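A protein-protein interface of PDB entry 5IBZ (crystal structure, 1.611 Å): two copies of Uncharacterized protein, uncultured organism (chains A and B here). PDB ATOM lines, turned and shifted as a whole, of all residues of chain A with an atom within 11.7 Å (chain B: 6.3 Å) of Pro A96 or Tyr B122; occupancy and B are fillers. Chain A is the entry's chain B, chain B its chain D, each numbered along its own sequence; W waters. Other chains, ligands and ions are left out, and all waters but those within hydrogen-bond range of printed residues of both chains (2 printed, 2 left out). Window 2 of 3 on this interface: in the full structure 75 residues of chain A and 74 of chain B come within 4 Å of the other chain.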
ATOM      1  N   THR A  79      16.060 -28.336  13.452  1.00  0.00           N
ATOM      2  CA  THR A  79      16.737 -27.853  14.651  1.00  0.00           C
ATOM      3  C   THR A  79      15.835 -26.993  15.505  1.00  0.00           C
ATOM      4  O   THR A  79      14.792 -26.557  15.055  1.00  0.00           O
ATOM      5  CB  THR A  79      17.946 -26.954  14.321  1.00  0.00           C
ATOM      6  OG1 THR A  79      17.447 -25.691  13.859  1.00  0.00           O
ATOM      7  CG2 THR A  79      18.843 -27.568  13.286  1.00  0.00           C
ATOM      8  N   GLY A  80      16.256 -26.715  16.729  1.00  0.00           N
ATOM      9  CA  GLY A  80      15.525 -25.764  17.557  1.00  0.00           C
ATOM     10  C   GLY A  80      15.433 -24.387  16.914  1.00  0.00           C
ATOM     11  O   GLY A  80      14.419 -23.697  17.048  1.00  0.00           O
ATOM     12  N   TYR A  83      12.404 -23.369  14.915  1.00  0.00           N
ATOM     13  CA  TYR A  83      11.168 -22.998  15.612  1.00  0.00           C
ATOM     14  C   TYR A  83      11.258 -21.582  16.148  1.00  0.00           C
ATOM     15  O   TYR A  83      10.245 -20.920  16.380  1.00  0.00           O
ATOM     16  CB  TYR A  83      10.879 -23.997  16.751  1.00  0.00           C
ATOM     17  CG  TYR A  83      10.687 -25.415  16.266  1.00  0.00           C
ATOM     18  CD1 TYR A  83       9.422 -25.891  15.895  1.00  0.00           C
ATOM     19  CD2 TYR A  83      11.755 -26.287  16.189  1.00  0.00           C
ATOM     20  CE1 TYR A  83       9.253 -27.201  15.453  1.00  0.00           C
ATOM     21  CE2 TYR A  83      11.596 -27.587  15.737  1.00  0.00           C
ATOM     22  CZ  TYR A  83      10.346 -28.036  15.373  1.00  0.00           C
ATOM     23  OH  TYR A  83      10.231 -29.344  14.942  1.00  0.00           O
ATOM     24  N   VAL A  84      12.478 -21.115  16.357  1.00  0.00           N
ATOM     25  CA  VAL A  84      12.677 -19.712  16.676  1.00  0.00           C
ATOM     26  C   VAL A  84      12.339 -18.883  15.443  1.00  0.00           C
ATOM     27  O   VAL A  84      11.680 -17.870  15.542  1.00  0.00           O
ATOM     28  CB  VAL A  84      14.110 -19.407  17.107  1.00  0.00           C
ATOM     29  CG1 VAL A  84      14.239 -17.940  17.493  1.00  0.00           C
ATOM     30  CG2 VAL A  84      14.557 -20.315  18.243  1.00  0.00           C
ATOM     31  N   ASP A  86      10.482 -19.859  12.776  1.00  0.00           N
ATOM     32  CA  ASP A  86       9.119 -20.140  12.326  1.00  0.00           C
ATOM     33  C   ASP A  86       8.405 -21.005  13.361  1.00  0.00           C
ATOM     34  O   ASP A  86       8.468 -22.228  13.294  1.00  0.00           O
ATOM     35  CB  ASP A  86       9.122 -20.856  10.976  1.00  0.00           C
ATOM     36  CG  ASP A  86       7.724 -21.239  10.521  1.00  0.00           C
ATOM     37  OD1 ASP A  86       6.761 -20.556  10.930  1.00  0.00           O
ATOM     38  OD2 ASP A  86       7.594 -22.230   9.774  1.00  0.00           O
ATOM     39  N   PRO A  87       7.752 -20.369  14.335  1.00  0.00           N
ATOM     40  CA  PRO A  87       7.090 -21.144  15.390  1.00  0.00           C
ATOM     41  C   PRO A  87       6.200 -22.269  14.848  1.00  0.00           C
ATOM     42  O   PRO A  87       6.046 -23.303  15.504  1.00  0.00           O
ATOM     43  CB  PRO A  87       6.266 -20.087  16.117  1.00  0.00           C
ATOM     44  CG  PRO A  87       7.049 -18.830  15.950  1.00  0.00           C
ATOM     45  CD  PRO A  87       7.680 -18.919  14.582  1.00  0.00           C
ATOM     46  N   GLY A  88       5.649 -22.076  13.653  1.00  0.00           N
ATOM     47  CA  GLY A  88       4.733 -23.040  13.070  1.00  0.00           C
ATOM     48  C   GLY A  88       5.388 -24.208  12.356  1.00  0.00           C
ATOM     49  O   GLY A  88       4.687 -25.017  11.744  1.00  0.00           O
ATOM     50  N   ALA A  89       6.715 -24.309  12.431  1.00  0.00           N
ATOM     51  CA  ALA A  89       7.435 -25.388  11.756  1.00  0.00           C
ATOM     52  C   ALA A  89       6.775 -26.727  12.066  1.00  0.00           C
ATOM     53  O   ALA A  89       6.594 -27.093  13.229  1.00  0.00           O
ATOM     54  CB  ALA A  89       8.911 -25.406  12.166  1.00  0.00           C
ATOM     55  N   SER A  90       6.407 -27.444  11.012  1.00  0.00           N
ATOM     56  CA  SER A  90       5.691 -28.704  11.156  1.00  0.00           C
ATOM     57  C   SER A  90       6.313 -29.778  10.271  1.00  0.00           C
ATOM     58  O   SER A  90       5.736 -30.154   9.248  1.00  0.00           O
ATOM     59  CB  SER A  90       4.212 -28.515  10.805  1.00  0.00           C
ATOM     60  N   PRO A  91       7.495 -30.282  10.663  1.00  0.00           N
ATOM     61  CA  PRO A  91       8.204 -31.301   9.875  1.00  0.00           C
ATOM     62  C   PRO A  91       7.513 -32.665   9.824  1.00  0.00           C
ATOM     63  O   PRO A  91       7.868 -33.465   8.951  1.00  0.00           O
ATOM     64  CB  PRO A  91       9.552 -31.420  10.589  1.00  0.00           C
ATOM     65  CG  PRO A  91       9.286 -30.964  11.986  1.00  0.00           C
ATOM     66  CD  PRO A  91       8.261 -29.878  11.856  1.00  0.00           C
ATOM     67  N   PHE A  92       6.571 -32.944  10.728  1.00  0.00           N
ATOM     68  CA  PHE A  92       5.864 -34.227  10.675  1.00  0.00           C
ATOM     69  C   PHE A  92       4.382 -34.368  11.131  1.00  0.00           C
ATOM     70  O   PHE A  92       4.029 -35.452  11.589  1.00  0.00           O
ATOM     71  CB  PHE A  92       6.678 -35.232  11.498  1.00  0.00           C
ATOM     72  N   GLY A  93       3.493 -33.375  11.040  1.00  0.00           N
ATOM     73  CA  GLY A  93       3.749 -31.976  10.764  1.00  0.00           C
ATOM     74  C   GLY A  93       3.194 -31.197  11.942  1.00  0.00           C
ATOM     75  O   GLY A  93       3.907 -30.951  12.919  1.00  0.00           O
ATOM     76  N   LYS A  94       1.914 -30.837  11.866  1.00  0.00           N
ATOM     77  CA  LYS A  94       1.266 -30.046  12.912  1.00  0.00           C
ATOM     78  C   LYS A  94       1.258 -30.788  14.250  1.00  0.00           C
ATOM     79  O   LYS A  94       0.624 -31.836  14.382  1.00  0.00           O
ATOM     80  CB  LYS A  94      -0.169 -29.690  12.501  1.00  0.00           C
ATOM     81  N   SER A  95       1.956 -30.232  15.240  1.00  0.00           N
ATOM     82  CA  SER A  95       2.089 -30.875  16.549  1.00  0.00           C
ATOM     83  C   SER A  95       2.580 -29.890  17.617  1.00  0.00           C
ATOM     84  O   SER A  95       3.368 -28.989  17.314  1.00  0.00           O
ATOM     85  CB  SER A  95       3.057 -32.057  16.458  1.00  0.00           C
ATOM     86  OG  SER A  95       3.154 -32.748  17.696  1.00  0.00           O
ATOM     87  N   PRO A  96       2.118 -30.052  18.872  1.00  0.00           N
ATOM     88  CA  PRO A  96       2.741 -29.230  19.916  1.00  0.00           C
ATOM     89  C   PRO A  96       4.164 -29.694  20.227  1.00  0.00           C
ATOM     90  O   PRO A  96       4.947 -28.907  20.753  1.00  0.00           O
ATOM     91  CB  PRO A  96       1.819 -29.409  21.127  1.00  0.00           C
ATOM     92  CG  PRO A  96       1.056 -30.664  20.874  1.00  0.00           C
ATOM     93  CD  PRO A  96       1.016 -30.887  19.388  1.00  0.00           C
ATOM     94  N   ILE A  97       4.494 -30.944  19.903  1.00  0.00           N
ATOM     95  CA  ILE A  97       5.844 -31.425  20.104  1.00  0.00           C
ATOM     96  C   ILE A  97       6.732 -30.889  18.990  1.00  0.00           C
ATOM     97  O   ILE A  97       6.352 -30.824  17.819  1.00  0.00           O
ATOM     98  CB  ILE A  97       5.895 -32.967  20.167  1.00  0.00           C
ATOM     99  CG1 ILE A  97       5.027 -33.474  21.326  1.00  0.00           C
ATOM    100  CG2 ILE A  97       7.321 -33.466  20.354  1.00  0.00           C
ATOM    101  CD1 ILE A  97       5.377 -32.870  22.686  1.00  0.00           C
ATOM    102  N   ARG A  98       7.911 -30.460  19.396  1.00  0.00           N
ATOM    103  CA  ARG A  98       8.912 -29.911  18.507  1.00  0.00           C
ATOM    104  C   ARG A  98      10.045 -30.915  18.506  1.00  0.00           C
ATOM    105  O   ARG A  98      10.304 -31.542  19.530  1.00  0.00           O
ATOM    106  CB  ARG A  98       9.356 -28.535  18.990  1.00  0.00           C
ATOM    107  CG  ARG A  98       8.195 -27.541  19.019  1.00  0.00           C
ATOM    108  CD  ARG A  98       8.579 -26.153  19.457  1.00  0.00           C
ATOM    109  NE  ARG A  98       7.440 -25.245  19.300  1.00  0.00           N
ATOM    110  CZ  ARG A  98       7.489 -23.921  19.441  1.00  0.00           C
ATOM    111  NH1 ARG A  98       8.626 -23.311  19.736  1.00  0.00           N
ATOM    112  NH2 ARG A  98       6.394 -23.197  19.280  1.00  0.00           N
ATOM    113  N   PHE A  99      10.670 -31.109  17.350  1.00  0.00           N
ATOM    114  CA  PHE A  99      11.701 -32.122  17.165  1.00  0.00           C
ATOM    115  C   PHE A  99      12.952 -31.543  16.524  1.00  0.00           C
ATOM    116  O   PHE A  99      12.890 -30.586  15.738  1.00  0.00           O
ATOM    117  CB  PHE A  99      11.190 -33.262  16.262  1.00  0.00           C
ATOM    118  CG  PHE A  99      10.271 -34.228  16.942  1.00  0.00           C
ATOM    119  CD1 PHE A  99      10.757 -35.130  17.876  1.00  0.00           C
ATOM    120  CD2 PHE A  99       8.921 -34.247  16.631  1.00  0.00           C
ATOM    121  CE1 PHE A  99       9.909 -36.028  18.503  1.00  0.00           C
ATOM    122  CE2 PHE A  99       8.062 -35.141  17.253  1.00  0.00           C
ATOM    123  CZ  PHE A  99       8.556 -36.034  18.187  1.00  0.00           C
ATOM    124  N   ALA A 100      14.090 -32.143  16.846  1.00  0.00           N
ATOM    125  CA  ALA A 100      15.320 -31.944  16.088  1.00  0.00           C
ATOM    126  C   ALA A 100      15.780 -33.318  15.630  1.00  0.00           C
ATOM    127  O   ALA A 100      15.723 -34.280  16.403  1.00  0.00           O
ATOM    128  CB  ALA A 100      16.399 -31.276  16.930  1.00  0.00           C
ATOM    129  N   LYS B  16       2.933 -30.956  34.429  1.00  0.00           N
ATOM    130  CA  LYS B  16       3.798 -30.121  35.252  1.00  0.00           C
ATOM    131  C   LYS B  16       4.875 -30.960  35.934  1.00  0.00           C
ATOM    132  O   LYS B  16       5.971 -30.467  36.188  1.00  0.00           O
ATOM    133  CB  LYS B  16       2.981 -29.362  36.303  1.00  0.00           C
ATOM    134  N   LEU B  17       4.545 -32.219  36.231  1.00  0.00           N
ATOM    135  CA  LEU B  17       5.506 -33.200  36.753  1.00  0.00           C
ATOM    136  C   LEU B  17       6.839 -33.106  36.025  1.00  0.00           C
ATOM    137  O   LEU B  17       6.875 -33.190  34.798  1.00  0.00           O
ATOM    138  CB  LEU B  17       4.955 -34.607  36.596  1.00  0.00           C
ATOM    139  CG  LEU B  17       5.815 -35.716  37.180  1.00  0.00           C
ATOM    140  CD1 LEU B  17       5.778 -35.639  38.707  1.00  0.00           C
ATOM    141  CD2 LEU B  17       5.329 -37.067  36.669  1.00  0.00           C
ATOM    142  N   GLY B 120      13.573 -33.693  21.376  1.00  0.00           N
ATOM    143  CA  GLY B 120      12.189 -33.289  21.386  1.00  0.00           C
ATOM    144  C   GLY B 120      11.813 -32.534  22.643  1.00  0.00           C
ATOM    145  O   GLY B 120      12.401 -32.725  23.681  1.00  0.00           O
ATOM    146  N   TRP B 121      10.807 -31.674  22.519  1.00  0.00           N
ATOM    147  CA  TRP B 121      10.341 -30.829  23.608  1.00  0.00           C
ATOM    148  C   TRP B 121       8.997 -30.234  23.206  1.00  0.00           C
ATOM    149  O   TRP B 121       8.426 -30.622  22.201  1.00  0.00           O
ATOM    150  CB  TRP B 121      11.356 -29.723  23.907  1.00  0.00           C
ATOM    151  CG  TRP B 121      11.559 -28.733  22.779  1.00  0.00           C
ATOM    152  CD1 TRP B 121      10.980 -27.500  22.659  1.00  0.00           C
ATOM    153  CD2 TRP B 121      12.399 -28.893  21.629  1.00  0.00           C
ATOM    154  NE1 TRP B 121      11.413 -26.877  21.507  1.00  0.00           N
ATOM    155  CE2 TRP B 121      12.281 -27.716  20.854  1.00  0.00           C
ATOM    156  CE3 TRP B 121      13.243 -29.914  21.181  1.00  0.00           C
ATOM    157  CZ2 TRP B 121      12.966 -27.542  19.651  1.00  0.00           C
ATOM    158  CZ3 TRP B 121      13.940 -29.735  19.994  1.00  0.00           C
ATOM    159  CH2 TRP B 121      13.790 -28.566  19.238  1.00  0.00           C
ATOM    160  N   TYR B 122       8.499 -29.275  23.977  1.00  0.00           N
ATOM    161  CA  TYR B 122       7.332 -28.512  23.556  1.00  0.00           C
ATOM    162  C   TYR B 122       7.556 -27.107  24.047  1.00  0.00           C
ATOM    163  O   TYR B 122       8.376 -26.870  24.937  1.00  0.00           O
ATOM    164  CB  TYR B 122       6.025 -29.099  24.098  1.00  0.00           C
ATOM    165  CG  TYR B 122       5.947 -29.255  25.598  1.00  0.00           C
ATOM    166  CD1 TYR B 122       5.542 -28.199  26.409  1.00  0.00           C
ATOM    167  CD2 TYR B 122       6.234 -30.468  26.205  1.00  0.00           C
ATOM    168  CE1 TYR B 122       5.452 -28.350  27.783  1.00  0.00           C
ATOM    169  CE2 TYR B 122       6.147 -30.628  27.570  1.00  0.00           C
ATOM    170  CZ  TYR B 122       5.751 -29.570  28.354  1.00  0.00           C
ATOM    171  OH  TYR B 122       5.657 -29.717  29.713  1.00  0.00           O
ATOM    172  N   GLY B 123       6.842 -26.161  23.461  1.00  0.00           N
ATOM    173  CA  GLY B 123       7.103 -24.771  23.746  1.00  0.00           C
ATOM    174  C   GLY B 123       8.516 -24.374  23.347  1.00  0.00           C
ATOM    175  O   GLY B 123       9.096 -24.954  22.430  1.00  0.00           O
ATOM    176  N   GLU B 124       9.058 -23.364  24.018  1.00  0.00           N
ATOM    177  CA  GLU B 124      10.316 -22.766  23.606  1.00  0.00           C
ATOM    178  C   GLU B 124      11.509 -23.268  24.421  1.00  0.00           C
ATOM    179  O   GLU B 124      12.633 -22.827  24.196  1.00  0.00           O
ATOM    180  CB  GLU B 124      10.220 -21.241  23.706  1.00  0.00           C
ATOM    181  CG  GLU B 124       9.201 -20.637  22.744  1.00  0.00           C
ATOM    182  CD  GLU B 124       9.225 -19.112  22.727  1.00  0.00           C
ATOM    183  OE1 GLU B 124       9.843 -18.510  23.624  1.00  0.00           O
ATOM    184  OE2 GLU B 124       8.631 -18.518  21.805  1.00  0.00           O
ATOM    185  N   SER B 125      11.253 -24.189  25.357  1.00  0.00           N
ATOM    186  CA  SER B 125      12.262 -24.688  26.296  1.00  0.00           C
ATOM    187  C   SER B 125      12.361 -26.197  26.299  1.00  0.00           C
ATOM    188  O   SER B 125      11.355 -26.909  26.229  1.00  0.00           O
ATOM    189  CB  SER B 125      11.954 -24.239  27.735  1.00  0.00           C
ATOM    190  OG  SER B 125      12.001 -22.828  27.863  1.00  0.00           O
ATOM    191  N   LEU B 126      13.595 -26.665  26.408  1.00  0.00           N
ATOM    192  CA  LEU B 126      13.897 -28.084  26.529  1.00  0.00           C
ATOM    193  C   LEU B 126      14.130 -28.398  28.008  1.00  0.00           C
ATOM    194  O   LEU B 126      13.959 -27.534  28.870  1.00  0.00           O
ATOM    195  CB  LEU B 126      15.123 -28.445  25.693  1.00  0.00           C
ATOM    196  CG  LEU B 126      14.958 -28.452  24.184  1.00  0.00           C
ATOM    197  CD1 LEU B 126      14.952 -27.046  23.578  1.00  0.00           C
ATOM    198  CD2 LEU B 126      16.079 -29.268  23.600  1.00  0.00           C
ATOM    199  N   GLU B 132      15.339 -23.387  23.119  1.00  0.00           N
ATOM    200  CA  GLU B 132      15.431 -24.114  21.854  1.00  0.00           C
ATOM    201  C   GLU B 132      16.420 -23.444  20.903  1.00  0.00           C
ATOM    202  O   GLU B 132      16.963 -24.110  20.004  1.00  0.00           O
ATOM    203  CB  GLU B 132      14.044 -24.249  21.207  1.00  0.00           C
ATOM    204  CG  GLU B 132      13.419 -22.911  20.805  1.00  0.00           C
ATOM    205  CD  GLU B 132      11.999 -23.032  20.299  1.00  0.00           C
ATOM    206  OE1 GLU B 132      11.493 -24.167  20.148  1.00  0.00           O
ATOM    207  OE2 GLU B 132      11.379 -21.969  20.021  1.00  0.00           O
ATOM    208  N   ALA B 264      -0.502 -35.458  18.241  1.00  0.00           N
ATOM    209  CA  ALA B 264      -0.273 -35.345  19.676  1.00  0.00           C
ATOM    210  C   ALA B 264       0.674 -36.442  20.145  1.00  0.00           C
ATOM    211  O   ALA B 264       0.470 -37.624  19.853  1.00  0.00           O
ATOM    212  CB  ALA B 264      -1.581 -35.418  20.439  1.00  0.00           C
ATOM    213  N   LEU B 265       1.707 -36.035  20.875  1.00  0.00           N
ATOM    214  CA  LEU B 265       2.727 -36.956  21.359  1.00  0.00           C
ATOM    215  C   LEU B 265       3.152 -36.549  22.748  1.00  0.00           C
ATOM    216  O   LEU B 265       4.325 -36.208  22.981  1.00  0.00           O
ATOM    217  CB  LEU B 265       3.928 -36.966  20.431  1.00  0.00           C
ATOM    218  CG  LEU B 265       3.717 -37.509  19.019  1.00  0.00           C
ATOM    219  CD1 LEU B 265       5.025 -37.416  18.254  1.00  0.00           C
ATOM    220  CD2 LEU B 265       3.227 -38.950  19.036  1.00  0.00           C
ATOM    221  N   PRO B 266       2.214 -36.600  23.689  1.00  0.00           N
ATOM    222  CA  PRO B 266       2.496 -36.114  25.034  1.00  0.00           C
ATOM    223  C   PRO B 266       3.639 -36.873  25.705  1.00  0.00           C
ATOM    224  O   PRO B 266       4.392 -36.268  26.446  1.00  0.00           O
ATOM    225  CB  PRO B 266       1.168 -36.325  25.772  1.00  0.00           C
ATOM    226  CG  PRO B 266       0.414 -37.316  24.958  1.00  0.00           C
ATOM    227  CD  PRO B 266       0.848 -37.133  23.556  1.00  0.00           C
ATOM    228  N   GLY B 269       7.081 -35.464  24.856  1.00  0.00           N
ATOM    229  CA  GLY B 269       7.296 -34.185  25.511  1.00  0.00           C
ATOM    230  C   GLY B 269       7.548 -34.325  26.996  1.00  0.00           C
ATOM    231  O   GLY B 269       8.447 -33.681  27.546  1.00  0.00           O
ATOM    232  N   ASN B 270       6.743 -35.155  27.660  1.00  0.00           N
ATOM    233  CA  ASN B 270       6.880 -35.327  29.095  1.00  0.00           C
ATOM    234  C   ASN B 270       8.180 -36.027  29.446  1.00  0.00           C
ATOM    235  O   ASN B 270       8.834 -35.640  30.398  1.00  0.00           O
ATOM    236  CB  ASN B 270       5.715 -36.120  29.680  1.00  0.00           C
ATOM    237  CG  ASN B 270       4.397 -35.352  29.660  1.00  0.00           C
ATOM    238  OD1 ASN B 270       3.332 -35.949  29.774  1.00  0.00           O
ATOM    239  ND2 ASN B 270       4.465 -34.035  29.529  1.00  0.00           N
ATOM    240  N   ARG B 273      11.452 -33.551  27.764  1.00  0.00           N
ATOM    241  CA  ARG B 273      11.569 -32.198  28.335  1.00  0.00           C
ATOM    242  C   ARG B 273      11.338 -32.149  29.838  1.00  0.00           C
ATOM    243  O   ARG B 273      12.083 -31.503  30.563  1.00  0.00           O
ATOM    244  CB  ARG B 273      10.585 -31.253  27.670  1.00  0.00           C
ATOM    245  CG  ARG B 273      10.478 -29.888  28.377  1.00  0.00           C
ATOM    246  CD  ARG B 273       9.332 -29.120  27.830  1.00  0.00           C
ATOM    247  NE  ARG B 273       9.290 -27.729  28.234  1.00  0.00           N
ATOM    248  CZ  ARG B 273       8.643 -27.253  29.286  1.00  0.00           C
ATOM    249  NH1 ARG B 273       8.016 -28.070  30.128  1.00  0.00           N
ATOM    250  NH2 ARG B 273       8.639 -25.939  29.511  1.00  0.00           N
ATOM    251  N   ASP B 274      10.285 -32.798  30.307  1.00  0.00           N
ATOM    252  CA  ASP B 274       9.920 -32.597  31.702  1.00  0.00           C
ATOM    253  C   ASP B 274      10.764 -33.480  32.629  1.00  0.00           C
ATOM    254  O   ASP B 274      11.256 -33.007  33.655  1.00  0.00           O
ATOM    255  CB  ASP B 274       8.424 -32.847  31.914  1.00  0.00           C
ATOM    256  CG  ASP B 274       7.564 -31.823  31.200  1.00  0.00           C
ATOM    257  OD1 ASP B 274       8.031 -30.676  31.035  1.00  0.00           O
ATOM    258  OD2 ASP B 274       6.437 -32.165  30.815  1.00  0.00           O
HETATM  259  O   HOH W   1       4.808 -26.485  21.416  1.00  0.00           O
HETATM  260  O   HOH W   2       6.622 -20.303  19.936  1.00  0.00           O
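The backbone carbonyl oxygen (O) of Trp B121 is in hydrogen-bond range of the backbone NH (N) of Arg A98.
The guanidinium group (NH1) of Arg A98 sits at hydrogen-bond distance from the backbone carbonyl oxygen (O) of Gly B123.
The guanidinium group (NH1) of Arg A98 lies within salt-bridge range of the side-chain carboxylate (OE1) of Glu B132 (3.0 Å).
The backbone NH (N) of Phe A99 sits at hydrogen-bond distance from the side-chain hydroxyl (OH) of Tyr A83, at 3.0 Å.
The side-chain hydroxyl (OG) of Ser A95 sits at hydrogen-bond distance from the backbone NH (N) of Ile A97, 3.1 Å away.
O of Gly B123 is in hydrogen-bond range of NE1 of Trp B121 (3.1 Å).
The side-chain carboxylate (OE1) of Glu B132 sits at hydrogen-bond distance from the indole nitrogen (NE1) of Trp B121 (3.0 Å).
O of Glu B124 sits at hydrogen-bond distance from N of Glu B132 (3.0 Å).
N of Asp B274 sits at hydrogen-bond distance from O of Gly B269.
CA of Gly A80 touches CH2 of Trp B121 (3.7 Å).
Tyr A83 touches Glu B132.
Val A84 touches Glu B132 (CG2 to CG, 3.8 Å).
Tyr B122 touches Pro A96 (CB to O, 3.5 Å).
Trp B121 touches Ile A97 (O to CA, 3.4 Å).
O of Leu B265 touches CG1 of Ile A97, 3.3 Å away.
CD1 of Ile A97 touches CA of Gly B269 (3.7 Å).
Arg A98 touches Gly B120.
Phe A99 touches Leu B265.
Ala A100 touches Trp B121.
Pro A96 touches one residue of chain B.
Of chain A, only Pro A96 (3.5 Å) comes within 4 Å of Tyr B122.
No residue of chain A comes within 4 Å of Lys B16.
Trp B121 touches just these residues of chain A: Gly A80 (3.7 Å), Tyr A83 (3.9 Å), Ile A97 (3.4 Å), Arg A98 (2.9 Å) and Ala A100 (3.97 Å).
No residue of chain A comes within 4 Å of Ser B125.
No residue of chain A comes within 4 Å of Leu B126.
No residue of chain A comes within 4 Å of Ala B264.
Gly B269 touches just one residue of chain A: Ile A97.
No residue of chain A comes within 4 Å of Asn B270.
No residue of chain A comes within 4 Å of Arg B273.
Of the printed residues of chain B, Tyr A83 touches Trp B121 and Glu B132.
Printed residues of chain B within 4 Å of Arg A98: Gly B120 (3.2 Å), Trp B121 (2.9 Å), Gly B123 (3.2 Å) and Glu B132 (3.0 Å).
Pro A87 touches none of the printed residues of chain B.
The nearest residue of chain B that does not touch Pro A96 is Trp B121 (4.1 Å).
The nearest residue of chain A that does not touch Tyr B122 is Ile A97 (4.1 Å).
Hydrophobic or aromatic side chains of chain A within 4 Å of the printed part of chain B: Tyr A83, Val A84, Ile A97 and Phe A99.
Of the 17 printed residues of chain B, 7 touch a printed residue of chain A.
Hydrophobic or aromatic side chains of chain B within 4 Å of the printed part of chain A: Trp B121, Tyr B122 and Leu B265.
Among the printed residues, 15 pairs touch across the chains.
Among the printed residues, Asp or Glu carboxylates within 4 Å of a Lys or Arg side-chain nitrogen of the other chain: Arg A98 with Glu B132 (3.0 Å).
No position is printed for both chains.
Of the 15 pairs that touch across the chains among the printed residues, none has its exchanged pair printed and touching as well.
Water W1 lies within hydrogen-bond range of O of Pro A96 (2.5 Å) and N of Gly B123 (2.9 Å).
Water W2 bridges the guanidinium group of Arg A98 (3.0 Å) and the side-chain carboxylate of Glu B124 (3.3 Å).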
